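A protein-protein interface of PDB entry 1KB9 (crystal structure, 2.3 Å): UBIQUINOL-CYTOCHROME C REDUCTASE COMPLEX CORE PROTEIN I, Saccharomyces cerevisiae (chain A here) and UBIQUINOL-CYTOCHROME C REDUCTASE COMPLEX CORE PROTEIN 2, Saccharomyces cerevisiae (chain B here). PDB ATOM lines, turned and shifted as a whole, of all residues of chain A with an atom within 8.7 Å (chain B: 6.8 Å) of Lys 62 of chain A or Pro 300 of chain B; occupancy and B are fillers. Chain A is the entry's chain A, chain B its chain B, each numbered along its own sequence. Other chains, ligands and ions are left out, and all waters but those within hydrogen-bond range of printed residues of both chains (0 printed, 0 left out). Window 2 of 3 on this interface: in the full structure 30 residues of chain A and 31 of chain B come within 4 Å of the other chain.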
ATOM      1  N   GLU A  55     -16.314 -17.513  -0.398  1.00  0.00           N
ATOM      2  CA  GLU A  55     -15.070 -17.979  -0.999  1.00  0.00           C
ATOM      3  C   GLU A  55     -14.833 -19.466  -0.765  1.00  0.00           C
ATOM      4  O   GLU A  55     -14.740 -20.240  -1.717  1.00  0.00           O
ATOM      5  CB  GLU A  55     -13.874 -17.184  -0.471  1.00  0.00           C
ATOM      6  CG  GLU A  55     -13.782 -15.757  -0.983  1.00  0.00           C
ATOM      7  CD  GLU A  55     -12.428 -15.130  -0.698  1.00  0.00           C
ATOM      8  OE1 GLU A  55     -12.151 -14.800   0.476  1.00  0.00           O
ATOM      9  OE2 GLU A  55     -11.633 -14.979  -1.652  1.00  0.00           O
ATOM     10  N   ASN A  56     -14.742 -19.861   0.501  1.00  0.00           N
ATOM     11  CA  ASN A  56     -14.502 -21.256   0.857  1.00  0.00           C
ATOM     12  C   ASN A  56     -15.654 -22.159   0.428  1.00  0.00           C
ATOM     13  O   ASN A  56     -15.448 -23.329   0.110  1.00  0.00           O
ATOM     14  CB  ASN A  56     -14.277 -21.382   2.365  1.00  0.00           C
ATOM     15  CG  ASN A  56     -13.739 -22.743   2.765  1.00  0.00           C
ATOM     16  OD1 ASN A  56     -12.629 -23.119   2.391  1.00  0.00           O
ATOM     17  ND2 ASN A  56     -14.522 -23.483   3.537  1.00  0.00           N
ATOM     18  N   SER A  57     -16.861 -21.603   0.399  1.00  0.00           N
ATOM     19  CA  SER A  57     -18.047 -22.361   0.022  1.00  0.00           C
ATOM     20  C   SER A  57     -18.120 -22.614  -1.485  1.00  0.00           C
ATOM     21  O   SER A  57     -18.603 -23.663  -1.914  1.00  0.00           O
ATOM     22  CB  SER A  57     -19.311 -21.645   0.514  1.00  0.00           C
ATOM     23  OG  SER A  57     -20.441 -22.502   0.493  1.00  0.00           O
ATOM     24  N   ALA A  58     -17.640 -21.661  -2.280  1.00  0.00           N
ATOM     25  CA  ALA A  58     -17.645 -21.790  -3.740  1.00  0.00           C
ATOM     26  C   ALA A  58     -16.637 -22.837  -4.212  1.00  0.00           C
ATOM     27  O   ALA A  58     -16.863 -23.521  -5.212  1.00  0.00           O
ATOM     28  CB  ALA A  58     -17.355 -20.445  -4.397  1.00  0.00           C
ATOM     29  N   VAL A  59     -15.525 -22.949  -3.488  1.00  0.00           N
ATOM     30  CA  VAL A  59     -14.477 -23.915  -3.808  1.00  0.00           C
ATOM     31  C   VAL A  59     -15.014 -25.331  -3.629  1.00  0.00           C
ATOM     32  O   VAL A  59     -14.655 -26.236  -4.382  1.00  0.00           O
ATOM     33  CB  VAL A  59     -13.228 -23.710  -2.913  1.00  0.00           C
ATOM     34  CG1 VAL A  59     -12.189 -24.790  -3.183  1.00  0.00           C
ATOM     35  CG2 VAL A  59     -12.627 -22.336  -3.164  1.00  0.00           C
ATOM     36  N   ALA A  60     -15.890 -25.511  -2.643  1.00  0.00           N
ATOM     37  CA  ALA A  60     -16.492 -26.814  -2.366  1.00  0.00           C
ATOM     38  C   ALA A  60     -17.671 -27.104  -3.296  1.00  0.00           C
ATOM     39  O   ALA A  60     -17.958 -28.262  -3.592  1.00  0.00           O
ATOM     40  CB  ALA A  60     -16.939 -26.889  -0.916  1.00  0.00           C
ATOM     41  N   ALA A  61     -18.343 -26.049  -3.752  1.00  0.00           N
ATOM     42  CA  ALA A  61     -19.492 -26.180  -4.645  1.00  0.00           C
ATOM     43  C   ALA A  61     -19.083 -26.637  -6.043  1.00  0.00           C
ATOM     44  O   ALA A  61     -19.823 -27.374  -6.700  1.00  0.00           O
ATOM     45  CB  ALA A  61     -20.250 -24.871  -4.717  1.00  0.00           C
ATOM     46  N   LYS A  62     -17.917 -26.181  -6.499  1.00  0.00           N
ATOM     47  CA  LYS A  62     -17.388 -26.566  -7.810  1.00  0.00           C
ATOM     48  C   LYS A  62     -17.141 -28.072  -7.790  1.00  0.00           C
ATOM     49  O   LYS A  62     -17.499 -28.790  -8.724  1.00  0.00           O
ATOM     50  CB  LYS A  62     -16.059 -25.851  -8.089  1.00  0.00           C
ATOM     51  CG  LYS A  62     -16.161 -24.372  -8.447  1.00  0.00           C
ATOM     52  CD  LYS A  62     -16.676 -24.162  -9.868  1.00  0.00           C
ATOM     53  CE  LYS A  62     -16.635 -22.687 -10.259  1.00  0.00           C
ATOM     54  NZ  LYS A  62     -17.130 -22.450 -11.645  1.00  0.00           N
ATOM     55  N   GLU A  63     -16.548 -28.530  -6.690  1.00  0.00           N
ATOM     56  CA  GLU A  63     -16.221 -29.934  -6.480  1.00  0.00           C
ATOM     57  C   GLU A  63     -17.470 -30.782  -6.204  1.00  0.00           C
ATOM     58  O   GLU A  63     -17.398 -32.013  -6.176  1.00  0.00           O
ATOM     59  CB  GLU A  63     -15.237 -30.059  -5.310  1.00  0.00           C
ATOM     60  CG  GLU A  63     -14.370 -31.310  -5.331  1.00  0.00           C
ATOM     61  CD  GLU A  63     -13.265 -31.246  -6.375  1.00  0.00           C
ATOM     62  OE1 GLU A  63     -12.143 -30.823  -6.025  1.00  0.00           O
ATOM     63  OE2 GLU A  63     -13.514 -31.623  -7.542  1.00  0.00           O
ATOM     64  N   GLY A  64     -18.607 -30.117  -6.007  1.00  0.00           N
ATOM     65  CA  GLY A  64     -19.852 -30.819  -5.733  1.00  0.00           C
ATOM     66  C   GLY A  64     -20.023 -31.224  -4.278  1.00  0.00           C
ATOM     67  O   GLY A  64     -20.632 -32.253  -3.977  1.00  0.00           O
ATOM     68  N   LEU A  65     -19.472 -30.413  -3.377  1.00  0.00           N
ATOM     69  CA  LEU A  65     -19.547 -30.655  -1.939  1.00  0.00           C
ATOM     70  C   LEU A  65     -20.394 -29.588  -1.237  1.00  0.00           C
ATOM     71  O   LEU A  65     -20.430 -28.433  -1.665  1.00  0.00           O
ATOM     72  CB  LEU A  65     -18.137 -30.678  -1.337  1.00  0.00           C
ATOM     73  CG  LEU A  65     -17.326 -31.978  -1.374  1.00  0.00           C
ATOM     74  CD1 LEU A  65     -17.284 -32.568  -2.769  1.00  0.00           C
ATOM     75  CD2 LEU A  65     -15.921 -31.712  -0.862  1.00  0.00           C
ATOM     76  N   ALA A  66     -21.084 -29.988  -0.170  1.00  0.00           N
ATOM     77  CA  ALA A  66     -21.924 -29.072   0.605  1.00  0.00           C
ATOM     78  C   ALA A  66     -21.342 -28.901   2.004  1.00  0.00           C
ATOM     79  O   ALA A  66     -20.926 -29.874   2.636  1.00  0.00           O
ATOM     80  CB  ALA A  66     -23.351 -29.593   0.684  1.00  0.00           C
ATOM     81  N   PHE A  93     -10.669 -31.314   0.982  1.00  0.00           N
ATOM     82  CA  PHE A  93     -11.200 -29.991   1.287  1.00  0.00           C
ATOM     83  C   PHE A  93     -11.116 -29.697   2.783  1.00  0.00           C
ATOM     84  O   PHE A  93     -10.998 -28.542   3.192  1.00  0.00           O
ATOM     85  CB  PHE A  93     -12.650 -29.881   0.809  1.00  0.00           C
ATOM     86  CG  PHE A  93     -13.196 -28.486   0.858  1.00  0.00           C
ATOM     87  CD1 PHE A  93     -12.908 -27.580  -0.156  1.00  0.00           C
ATOM     88  CD2 PHE A  93     -13.977 -28.066   1.928  1.00  0.00           C
ATOM     89  CE1 PHE A  93     -13.386 -26.274  -0.102  1.00  0.00           C
ATOM     90  CE2 PHE A  93     -14.459 -26.763   1.991  1.00  0.00           C
ATOM     91  CZ  PHE A  93     -14.161 -25.866   0.973  1.00  0.00           C
ATOM     92  N   TYR B 243     -28.114 -23.330  -8.430  1.00  0.00           N
ATOM     93  CA  TYR B 243     -27.019 -22.465  -8.852  1.00  0.00           C
ATOM     94  C   TYR B 243     -27.242 -21.104  -8.198  1.00  0.00           C
ATOM     95  O   TYR B 243     -26.336 -20.552  -7.574  1.00  0.00           O
ATOM     96  CB  TYR B 243     -26.997 -22.342 -10.385  1.00  0.00           C
ATOM     97  CG  TYR B 243     -26.122 -21.232 -10.940  1.00  0.00           C
ATOM     98  CD1 TYR B 243     -24.729 -21.290 -10.845  1.00  0.00           C
ATOM     99  CD2 TYR B 243     -26.696 -20.117 -11.558  1.00  0.00           C
ATOM    100  CE1 TYR B 243     -23.928 -20.260 -11.352  1.00  0.00           C
ATOM    101  CE2 TYR B 243     -25.908 -19.084 -12.067  1.00  0.00           C
ATOM    102  CZ  TYR B 243     -24.528 -19.159 -11.960  1.00  0.00           C
ATOM    103  OH  TYR B 243     -23.760 -18.122 -12.445  1.00  0.00           O
ATOM    104  N   LEU B 248     -21.549 -20.364  -5.912  1.00  0.00           N
ATOM    105  CA  LEU B 248     -21.058 -20.261  -7.283  1.00  0.00           C
ATOM    106  C   LEU B 248     -21.579 -18.998  -7.954  1.00  0.00           C
ATOM    107  O   LEU B 248     -20.819 -18.272  -8.596  1.00  0.00           O
ATOM    108  CB  LEU B 248     -21.466 -21.495  -8.088  1.00  0.00           C
ATOM    109  CG  LEU B 248     -20.914 -22.812  -7.539  1.00  0.00           C
ATOM    110  CD1 LEU B 248     -21.392 -23.974  -8.381  1.00  0.00           C
ATOM    111  CD2 LEU B 248     -19.398 -22.765  -7.507  1.00  0.00           C
ATOM    112  N   ASP B 297     -24.225 -20.488 -17.670  1.00  0.00           N
ATOM    113  CA  ASP B 297     -24.192 -21.595 -16.721  1.00  0.00           C
ATOM    114  C   ASP B 297     -22.869 -22.349 -16.821  1.00  0.00           C
ATOM    115  O   ASP B 297     -22.038 -22.262 -15.919  1.00  0.00           O
ATOM    116  CB  ASP B 297     -25.368 -22.551 -16.965  1.00  0.00           C
ATOM    117  CG  ASP B 297     -25.664 -23.441 -15.766  1.00  0.00           C
ATOM    118  OD1 ASP B 297     -24.838 -24.321 -15.444  1.00  0.00           O
ATOM    119  OD2 ASP B 297     -26.734 -23.263 -15.148  1.00  0.00           O
ATOM    120  N   LEU B 298     -22.679 -23.054 -17.938  1.00  0.00           N
ATOM    121  CA  LEU B 298     -21.479 -23.855 -18.213  1.00  0.00           C
ATOM    122  C   LEU B 298     -21.377 -25.100 -17.327  1.00  0.00           C
ATOM    123  O   LEU B 298     -20.341 -25.766 -17.289  1.00  0.00           O
ATOM    124  CB  LEU B 298     -20.201 -23.007 -18.108  1.00  0.00           C
ATOM    125  CG  LEU B 298     -20.018 -21.892 -19.144  1.00  0.00           C
ATOM    126  CD1 LEU B 298     -18.737 -21.125 -18.854  1.00  0.00           C
ATOM    127  CD2 LEU B 298     -19.989 -22.479 -20.550  1.00  0.00           C
ATOM    128  N   SER B 299     -22.471 -25.400 -16.627  1.00  0.00           N
ATOM    129  CA  SER B 299     -22.599 -26.554 -15.733  1.00  0.00           C
ATOM    130  C   SER B 299     -21.514 -26.782 -14.674  1.00  0.00           C
ATOM    131  O   SER B 299     -20.995 -27.892 -14.539  1.00  0.00           O
ATOM    132  CB  SER B 299     -22.815 -27.837 -16.549  1.00  0.00           C
ATOM    133  OG  SER B 299     -21.725 -28.096 -17.420  1.00  0.00           O
ATOM    134  N   PRO B 300     -21.165 -25.742 -13.897  1.00  0.00           N
ATOM    135  CA  PRO B 300     -20.136 -25.907 -12.864  1.00  0.00           C
ATOM    136  C   PRO B 300     -20.760 -26.605 -11.658  1.00  0.00           C
ATOM    137  O   PRO B 300     -20.093 -27.345 -10.930  1.00  0.00           O
ATOM    138  CB  PRO B 300     -19.763 -24.460 -12.514  1.00  0.00           C
ATOM    139  CG  PRO B 300     -20.285 -23.642 -13.679  1.00  0.00           C
ATOM    140  CD  PRO B 300     -21.573 -24.334 -13.984  1.00  0.00           C
ATOM    141  N   ALA B 301     -22.055 -26.354 -11.471  1.00  0.00           N
ATOM    142  CA  ALA B 301     -22.834 -26.919 -10.375  1.00  0.00           C
ATOM    143  C   ALA B 301     -23.552 -28.198 -10.791  1.00  0.00           C
ATOM    144  O   ALA B 301     -24.584 -28.544 -10.221  1.00  0.00           O
ATOM    145  CB  ALA B 301     -23.848 -25.892  -9.881  1.00  0.00           C
ATOM    146  N   ILE B 302     -23.002 -28.895 -11.779  1.00  0.00           N
ATOM    147  CA  ILE B 302     -23.596 -30.135 -12.271  1.00  0.00           C
ATOM    148  C   ILE B 302     -23.526 -31.246 -11.219  1.00  0.00           C
ATOM    149  O   ILE B 302     -24.412 -32.102 -11.144  1.00  0.00           O
ATOM    150  CB  ILE B 302     -22.919 -30.598 -13.590  1.00  0.00           C
ATOM    151  CG1 ILE B 302     -23.740 -31.711 -14.243  1.00  0.00           C
ATOM    152  CG2 ILE B 302     -21.483 -31.051 -13.335  1.00  0.00           C
ATOM    153  CD1 ILE B 302     -25.135 -31.278 -14.633  1.00  0.00           C
ATOM    154  N   ASN B 303     -22.475 -31.217 -10.404  1.00  0.00           N
ATOM    155  CA  ASN B 303     -22.289 -32.208  -9.352  1.00  0.00           C
ATOM    156  C   ASN B 303     -22.944 -31.736  -8.061  1.00  0.00           C
ATOM    157  O   ASN B 303     -23.318 -32.547  -7.214  1.00  0.00           O
ATOM    158  CB  ASN B 303     -20.800 -32.471  -9.122  1.00  0.00           C
ATOM    159  CG  ASN B 303     -20.112 -33.034 -10.350  1.00  0.00           C
ATOM    160  OD1 ASN B 303     -20.486 -34.092 -10.857  1.00  0.00           O
ATOM    161  ND2 ASN B 303     -19.100 -32.326 -10.837  1.00  0.00           N
ATOM    162  N   TYR B 304     -23.074 -30.419  -7.916  1.00  0.00           N
ATOM    163  CA  TYR B 304     -23.691 -29.825  -6.736  1.00  0.00           C
ATOM    164  C   TYR B 304     -25.206 -29.998  -6.782  1.00  0.00           C
ATOM    165  O   TYR B 304     -25.817 -30.386  -5.788  1.00  0.00           O
ATOM    166  CB  TYR B 304     -23.330 -28.339  -6.630  1.00  0.00           C
ATOM    167  CG  TYR B 304     -23.879 -27.647  -5.397  1.00  0.00           C
ATOM    168  CD1 TYR B 304     -24.882 -26.681  -5.503  1.00  0.00           C
ATOM    169  CD2 TYR B 304     -23.390 -27.950  -4.124  1.00  0.00           C
ATOM    170  CE1 TYR B 304     -25.383 -26.034  -4.376  1.00  0.00           C
ATOM    171  CE2 TYR B 304     -23.886 -27.309  -2.988  1.00  0.00           C
ATOM    172  CZ  TYR B 304     -24.881 -26.352  -3.123  1.00  0.00           C
ATOM    173  OH  TYR B 304     -25.373 -25.711  -2.008  1.00  0.00           O
ATOM    174  N   LYS B 328     -26.483 -27.588 -20.482  1.00  0.00           N
ATOM    175  CA  LYS B 328     -25.613 -26.799 -19.618  1.00  0.00           C
ATOM    176  C   LYS B 328     -25.714 -25.294 -19.871  1.00  0.00           C
ATOM    177  O   LYS B 328     -24.856 -24.529 -19.430  1.00  0.00           O
ATOM    178  CB  LYS B 328     -24.159 -27.248 -19.780  1.00  0.00           C
ATOM    179  CG  LYS B 328     -23.551 -26.924 -21.137  1.00  0.00           C
ATOM    180  CD  LYS B 328     -22.035 -26.992 -21.082  1.00  0.00           C
ATOM    181  CE  LYS B 328     -21.411 -26.415 -22.342  1.00  0.00           C
ATOM    182  NZ  LYS B 328     -19.932 -26.319 -22.223  1.00  0.00           N
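The backbone NH of Leu 65 of chain A lies within hydrogen-bond range of the backbone carbonyl oxygen of Ala 60 of chain A.
Among the printed residues, pairs that only touch across the chains: Ala 58 of chain A with Leu 248 of chain B (3.5 Å), Ala 61 of chain A with Leu 248 of chain B (3.6 Å), Ala 61 of chain A with Tyr 304 of chain B (3.6 Å), Lys 62 of chain A with Leu 248 of chain B (3.7 Å), Lys 62 of chain A with Pro 300 of chain B (3.4 Å), Gly 64 of chain A with Asn 303 of chain B (3.9 Å), Gly 64 of chain A with Tyr 304 of chain B (3.9 Å) and Leu 65 of chain A with Tyr 304 of chain B (3.9 Å).
Printed residues of chain B within 4 Å of Ala 61 of chain A: Leu 248 (3.6 Å) and Tyr 304 (3.6 Å).
Lys 62 of chain A touches just these residues of chain B: Leu 248 and Pro 300.
Of the printed residues of chain B, Gly 64 of chain A touches Asn 303 and Tyr 304.
Tyr 243 of chain B touches none of the printed residues of chain A.
No residue of chain A comes within 4 Å of Ser 299 of chain B.
Of the printed residues of chain A, Pro 300 of chain B touches Lys 62.
No residue of chain A comes within 4 Å of Ala 301 of chain B.
The nearest residue of chain B that does not touch Lys 62 of chain A is Asn 303 of chain B (4.4 Å).
The nearest printed residue of chain A that does not touch Asn 303 of chain B is Lys 62 of chain A (4.4 Å).
Of the 13 printed residues of chain A, 5 touch a printed residue of chain B.
Printed residues of chain A that touch a printed residue of chain B: Ala 58, Ala 61, Lys 62, Gly 64 and Leu 65.
Hydrophobic or aromatic side chains of chain A within 4 Å of the printed part of chain B: Ala 61.
Printed residues of chain B that touch a printed residue of chain A: Leu 248, Pro 300, Asn 303 and Tyr 304.
Hydrophobic or aromatic side chains of chain B that line the printed part of chain A: Leu 248, Pro 300 and Tyr 304.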
